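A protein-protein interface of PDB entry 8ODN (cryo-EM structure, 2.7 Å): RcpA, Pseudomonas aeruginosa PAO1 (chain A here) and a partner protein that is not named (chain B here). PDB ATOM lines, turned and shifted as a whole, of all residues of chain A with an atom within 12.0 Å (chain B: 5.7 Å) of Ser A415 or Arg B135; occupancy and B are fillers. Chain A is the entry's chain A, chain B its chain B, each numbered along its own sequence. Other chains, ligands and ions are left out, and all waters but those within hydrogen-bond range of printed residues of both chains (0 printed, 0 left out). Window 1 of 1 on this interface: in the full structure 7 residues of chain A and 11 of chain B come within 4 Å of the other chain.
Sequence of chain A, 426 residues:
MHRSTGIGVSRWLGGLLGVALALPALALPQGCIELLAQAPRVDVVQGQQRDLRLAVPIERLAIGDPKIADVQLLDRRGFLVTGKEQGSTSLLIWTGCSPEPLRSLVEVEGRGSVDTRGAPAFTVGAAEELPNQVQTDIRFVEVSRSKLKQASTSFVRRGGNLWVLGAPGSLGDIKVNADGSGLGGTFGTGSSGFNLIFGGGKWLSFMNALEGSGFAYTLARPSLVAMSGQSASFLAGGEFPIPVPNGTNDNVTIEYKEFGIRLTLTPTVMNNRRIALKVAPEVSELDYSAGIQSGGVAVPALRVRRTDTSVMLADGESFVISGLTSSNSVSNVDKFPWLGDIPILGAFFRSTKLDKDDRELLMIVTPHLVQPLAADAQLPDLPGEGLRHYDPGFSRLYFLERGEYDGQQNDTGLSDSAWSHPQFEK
Among the printed residues, merely in contact across the chains: Ser A415 with Arg B135, Leu A414 with Leu B169, Leu A414 with Asp B139 and Ser A415 with Leu B169.
Ser A415 touches just these residues of chain B: Arg B135, Asp B139 and Leu B169. Glu B101 touches none of the printed residues of chain A. No residue of chain A comes within 4 Å of Glu B133. Asn B138 touches none of the printed residues of chain A. Of the printed residues of chain A, Leu B169 touches Leu A414 and Ser A415. Printed residues of chain B within 4 Å of Leu A414: Asp B139 and Leu B169. Arg B137 touches none of the printed residues of chain A. His B104 touches none of the printed residues of chain A. The nearest residue of chain B that does not touch Ser A415 is Asn B138 (5.1 Å). The nearest residue of chain A that does not touch Arg B135 is Asp A416 (6.2 Å). The nearest printed residue of chain A that does not touch Leu B169 is Gly A413 (4.4 Å).
Of the 5 printed residues of chain A, 2 touch a printed residue of chain B. Hydrophobic or aromatic side chains of chain A that line the printed part of chain B: Leu A414. Of the 11 printed residues of chain B, 3 touch a printed residue of chain A. Among the printed residues, 5 pairs touch across the chains.
A ring nitrogen (NE2) of His B104 sits at hydrogen-bond distance from the side-chain carboxylate (OD2) of Asp B139 (2.6 Å). OE2 of Glu B133 is in salt-bridge range of NH2 of Arg B135, 2.6 Å away.
The backbone NH (N) of Ser A415 lies within hydrogen-bond range of the side-chain carboxylate (OD1) of Asp B139.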
ATOM      1  N   THR A 412      -9.482   3.421 -33.265  1.00  0.00           N
ATOM      2  CA  THR A 412     -10.577   4.305 -32.885  1.00  0.00           C
ATOM      3  C   THR A 412     -10.098   5.395 -31.930  1.00  0.00           C
ATOM      4  O   THR A 412     -10.827   6.346 -31.650  1.00  0.00           O
ATOM      5  CB  THR A 412     -11.730   3.522 -32.217  1.00  0.00           C
ATOM      6  OG1 THR A 412     -11.261   2.898 -31.015  1.00  0.00           O
ATOM      7  CG2 THR A 412     -12.281   2.460 -33.162  1.00  0.00           C
ATOM      8  N   GLY A 413      -8.872   5.253 -31.428  1.00  0.00           N
ATOM      9  CA  GLY A 413      -8.282   6.214 -30.527  1.00  0.00           C
ATOM     10  C   GLY A 413      -8.413   5.854 -29.064  1.00  0.00           C
ATOM     11  O   GLY A 413      -7.693   6.418 -28.233  1.00  0.00           O
ATOM     12  N   LEU A 414      -9.316   4.935 -28.729  1.00  0.00           N
ATOM     13  CA  LEU A 414      -9.486   4.524 -27.348  1.00  0.00           C
ATOM     14  C   LEU A 414      -8.273   3.723 -26.874  1.00  0.00           C
ATOM     15  O   LEU A 414      -7.480   3.203 -27.666  1.00  0.00           O
ATOM     16  CB  LEU A 414     -10.767   3.705 -27.187  1.00  0.00           C
ATOM     17  CG  LEU A 414     -12.076   4.474 -27.403  1.00  0.00           C
ATOM     18  CD1 LEU A 414     -13.225   3.510 -27.638  1.00  0.00           C
ATOM     19  CD2 LEU A 414     -12.380   5.381 -26.218  1.00  0.00           C
ATOM     20  N   SER A 415      -8.143   3.623 -25.549  1.00  0.00           N
ATOM     21  CA  SER A 415      -6.992   2.957 -24.949  1.00  0.00           C
ATOM     22  C   SER A 415      -6.950   1.467 -25.261  1.00  0.00           C
ATOM     23  O   SER A 415      -5.865   0.877 -25.256  1.00  0.00           O
ATOM     24  CB  SER A 415      -6.998   3.160 -23.433  1.00  0.00           C
ATOM     25  OG  SER A 415      -5.911   2.489 -22.812  1.00  0.00           O
ATOM     26  N   ASP A 416      -8.094   0.855 -25.539  1.00  0.00           N
ATOM     27  CA  ASP A 416      -8.591  -0.477 -25.854  1.00  0.00           C
ATOM     28  C   ASP A 416      -8.728  -1.305 -24.582  1.00  0.00           C
ATOM     29  O   ASP A 416      -9.811  -1.392 -24.006  1.00  0.00           O
ATOM     30  CB  ASP A 416      -7.661  -1.180 -26.848  1.00  0.00           C
ATOM     31  CG  ASP A 416      -7.406  -0.350 -28.090  1.00  0.00           C
ATOM     32  OD1 ASP A 416      -8.371   0.249 -28.613  1.00  0.00           O
ATOM     33  OD2 ASP A 416      -6.243  -0.285 -28.539  1.00  0.00           O
ATOM     34  N   GLU B 101     -13.247   2.061 -11.758  1.00  0.00           N
ATOM     35  CA  GLU B 101     -13.005   1.191 -12.901  1.00  0.00           C
ATOM     36  C   GLU B 101     -14.276   0.494 -13.363  1.00  0.00           C
ATOM     37  O   GLU B 101     -14.394   0.165 -14.544  1.00  0.00           O
ATOM     38  CB  GLU B 101     -11.934   0.151 -12.566  1.00  0.00           C
ATOM     39  CG  GLU B 101     -10.528   0.716 -12.437  1.00  0.00           C
ATOM     40  CD  GLU B 101      -9.508  -0.352 -12.090  1.00  0.00           C
ATOM     41  OE1 GLU B 101      -9.918  -1.500 -11.824  1.00  0.00           O
ATOM     42  OE2 GLU B 101      -8.297  -0.045 -12.089  1.00  0.00           O
ATOM     43  N   HIS B 104     -15.896   3.066 -15.511  1.00  0.00           N
ATOM     44  CA  HIS B 104     -15.131   3.139 -16.752  1.00  0.00           C
ATOM     45  C   HIS B 104     -15.413   1.943 -17.656  1.00  0.00           C
ATOM     46  O   HIS B 104     -15.509   2.091 -18.880  1.00  0.00           O
ATOM     47  CB  HIS B 104     -13.641   3.237 -16.433  1.00  0.00           C
ATOM     48  CG  HIS B 104     -12.763   3.143 -17.639  1.00  0.00           C
ATOM     49  ND1 HIS B 104     -12.067   1.999 -17.964  1.00  0.00           N
ATOM     50  CD2 HIS B 104     -12.468   4.049 -18.601  1.00  0.00           C
ATOM     51  CE1 HIS B 104     -11.378   2.206 -19.072  1.00  0.00           C
ATOM     52  NE2 HIS B 104     -11.606   3.441 -19.479  1.00  0.00           N
ATOM     53  N   GLU B 133      -6.101   9.119 -13.471  1.00  0.00           N
ATOM     54  CA  GLU B 133      -5.994   8.017 -14.418  1.00  0.00           C
ATOM     55  C   GLU B 133      -5.946   8.543 -15.848  1.00  0.00           C
ATOM     56  O   GLU B 133      -6.961   8.989 -16.390  1.00  0.00           O
ATOM     57  CB  GLU B 133      -7.162   7.043 -14.255  1.00  0.00           C
ATOM     58  CG  GLU B 133      -6.953   5.736 -15.006  1.00  0.00           C
ATOM     59  CD  GLU B 133      -5.758   4.963 -14.484  1.00  0.00           C
ATOM     60  OE1 GLU B 133      -5.367   5.193 -13.320  1.00  0.00           O
ATOM     61  OE2 GLU B 133      -5.201   4.136 -15.238  1.00  0.00           O
ATOM     62  N   SER B 134      -4.760   8.490 -16.463  1.00  0.00           N
ATOM     63  CA  SER B 134      -4.597   8.963 -17.836  1.00  0.00           C
ATOM     64  C   SER B 134      -5.519   8.210 -18.785  1.00  0.00           C
ATOM     65  O   SER B 134      -6.094   8.796 -19.711  1.00  0.00           O
ATOM     66  CB  SER B 134      -3.138   8.807 -18.270  1.00  0.00           C
ATOM     67  OG  SER B 134      -2.953   9.214 -19.615  1.00  0.00           O
ATOM     68  N   ARG B 135      -5.650   6.898 -18.587  1.00  0.00           N
ATOM     69  CA  ARG B 135      -6.520   6.096 -19.442  1.00  0.00           C
ATOM     70  C   ARG B 135      -7.958   6.605 -19.408  1.00  0.00           C
ATOM     71  O   ARG B 135      -8.600   6.753 -20.457  1.00  0.00           O
ATOM     72  CB  ARG B 135      -6.452   4.632 -18.998  1.00  0.00           C
ATOM     73  CG  ARG B 135      -7.263   3.659 -19.851  1.00  0.00           C
ATOM     74  CD  ARG B 135      -6.850   2.209 -19.592  1.00  0.00           C
ATOM     75  NE  ARG B 135      -6.111   2.055 -18.345  1.00  0.00           N
ATOM     76  CZ  ARG B 135      -6.658   1.994 -17.142  1.00  0.00           C
ATOM     77  NH1 ARG B 135      -7.963   2.105 -16.973  1.00  0.00           N
ATOM     78  NH2 ARG B 135      -5.871   1.824 -16.083  1.00  0.00           N
ATOM     79  N   PHE B 136      -8.477   6.893 -18.211  1.00  0.00           N
ATOM     80  CA  PHE B 136      -9.835   7.414 -18.090  1.00  0.00           C
ATOM     81  C   PHE B 136      -9.982   8.742 -18.820  1.00  0.00           C
ATOM     82  O   PHE B 136     -10.975   8.971 -19.518  1.00  0.00           O
ATOM     83  CB  PHE B 136     -10.204   7.591 -16.616  1.00  0.00           C
ATOM     84  CG  PHE B 136     -10.332   6.304 -15.850  1.00  0.00           C
ATOM     85  CD1 PHE B 136     -10.224   5.077 -16.481  1.00  0.00           C
ATOM     86  CD2 PHE B 136     -10.567   6.329 -14.486  1.00  0.00           C
ATOM     87  CE1 PHE B 136     -10.343   3.904 -15.767  1.00  0.00           C
ATOM     88  CE2 PHE B 136     -10.688   5.157 -13.768  1.00  0.00           C
ATOM     89  CZ  PHE B 136     -10.579   3.945 -14.411  1.00  0.00           C
ATOM     90  N   ARG B 137      -9.011   9.642 -18.647  1.00  0.00           N
ATOM     91  CA  ARG B 137      -9.091  10.953 -19.284  1.00  0.00           C
ATOM     92  C   ARG B 137      -9.054  10.832 -20.802  1.00  0.00           C
ATOM     93  O   ARG B 137      -9.823  11.500 -21.505  1.00  0.00           O
ATOM     94  CB  ARG B 137      -7.952  11.838 -18.779  1.00  0.00           C
ATOM     95  CG  ARG B 137      -8.068  12.209 -17.309  1.00  0.00           C
ATOM     96  CD  ARG B 137      -9.123  13.277 -17.087  1.00  0.00           C
ATOM     97  NE  ARG B 137      -9.653  13.256 -15.728  1.00  0.00           N
ATOM     98  CZ  ARG B 137     -10.500  14.154 -15.241  1.00  0.00           C
ATOM     99  NH1 ARG B 137     -10.919  15.178 -15.967  1.00  0.00           N
ATOM    100  NH2 ARG B 137     -10.938  14.020 -13.993  1.00  0.00           N
ATOM    101  N   ASN B 138      -8.171   9.980 -21.328  1.00  0.00           N
ATOM    102  CA  ASN B 138      -8.068   9.829 -22.772  1.00  0.00           C
ATOM    103  C   ASN B 138      -9.287   9.140 -23.365  1.00  0.00           C
ATOM    104  O   ASN B 138      -9.628   9.404 -24.522  1.00  0.00           O
ATOM    105  CB  ASN B 138      -6.811   9.043 -23.137  1.00  0.00           C
ATOM    106  CG  ASN B 138      -6.488   9.122 -24.615  1.00  0.00           C
ATOM    107  OD1 ASN B 138      -6.869  10.077 -25.293  1.00  0.00           O
ATOM    108  ND2 ASN B 138      -5.789   8.117 -25.124  1.00  0.00           N
ATOM    109  N   ASP B 139      -9.952   8.268 -22.603  1.00  0.00           N
ATOM    110  CA  ASP B 139     -11.196   7.679 -23.087  1.00  0.00           C
ATOM    111  C   ASP B 139     -12.344   8.681 -23.037  1.00  0.00           C
ATOM    112  O   ASP B 139     -13.156   8.751 -23.969  1.00  0.00           O
ATOM    113  CB  ASP B 139     -11.544   6.439 -22.266  1.00  0.00           C
ATOM    114  CG  ASP B 139     -10.482   5.360 -22.357  1.00  0.00           C
ATOM    115  OD1 ASP B 139      -9.809   5.271 -23.405  1.00  0.00           O
ATOM    116  OD2 ASP B 139     -10.322   4.601 -21.378  1.00  0.00           O
ATOM    117  N   LEU B 140     -12.436   9.453 -21.953  1.00  0.00           N
ATOM    118  CA  LEU B 140     -13.491  10.452 -21.840  1.00  0.00           C
ATOM    119  C   LEU B 140     -13.356  11.519 -22.920  1.00  0.00           C
ATOM    120  O   LEU B 140     -14.363  12.000 -23.452  1.00  0.00           O
ATOM    121  CB  LEU B 140     -13.464  11.083 -20.448  1.00  0.00           C
ATOM    122  CG  LEU B 140     -14.403  12.267 -20.201  1.00  0.00           C
ATOM    123  CD1 LEU B 140     -15.849  11.936 -20.538  1.00  0.00           C
ATOM    124  CD2 LEU B 140     -14.280  12.714 -18.755  1.00  0.00           C
ATOM    125  N   LEU B 169      -1.044   7.853 -27.274  1.00  0.00           N
ATOM    126  CA  LEU B 169      -2.406   7.958 -27.769  1.00  0.00           C
ATOM    127  C   LEU B 169      -2.922   9.374 -27.532  1.00  0.00           C
ATOM    128  O   LEU B 169      -3.512   9.967 -28.441  1.00  0.00           O
ATOM    129  CB  LEU B 169      -3.305   6.908 -27.112  1.00  0.00           C
ATOM    130  CG  LEU B 169      -3.122   5.467 -27.612  1.00  0.00           C
ATOM    131  CD1 LEU B 169      -4.033   4.482 -26.880  1.00  0.00           C
ATOM    132  CD2 LEU B 169      -3.346   5.350 -29.117  1.00  0.00           C
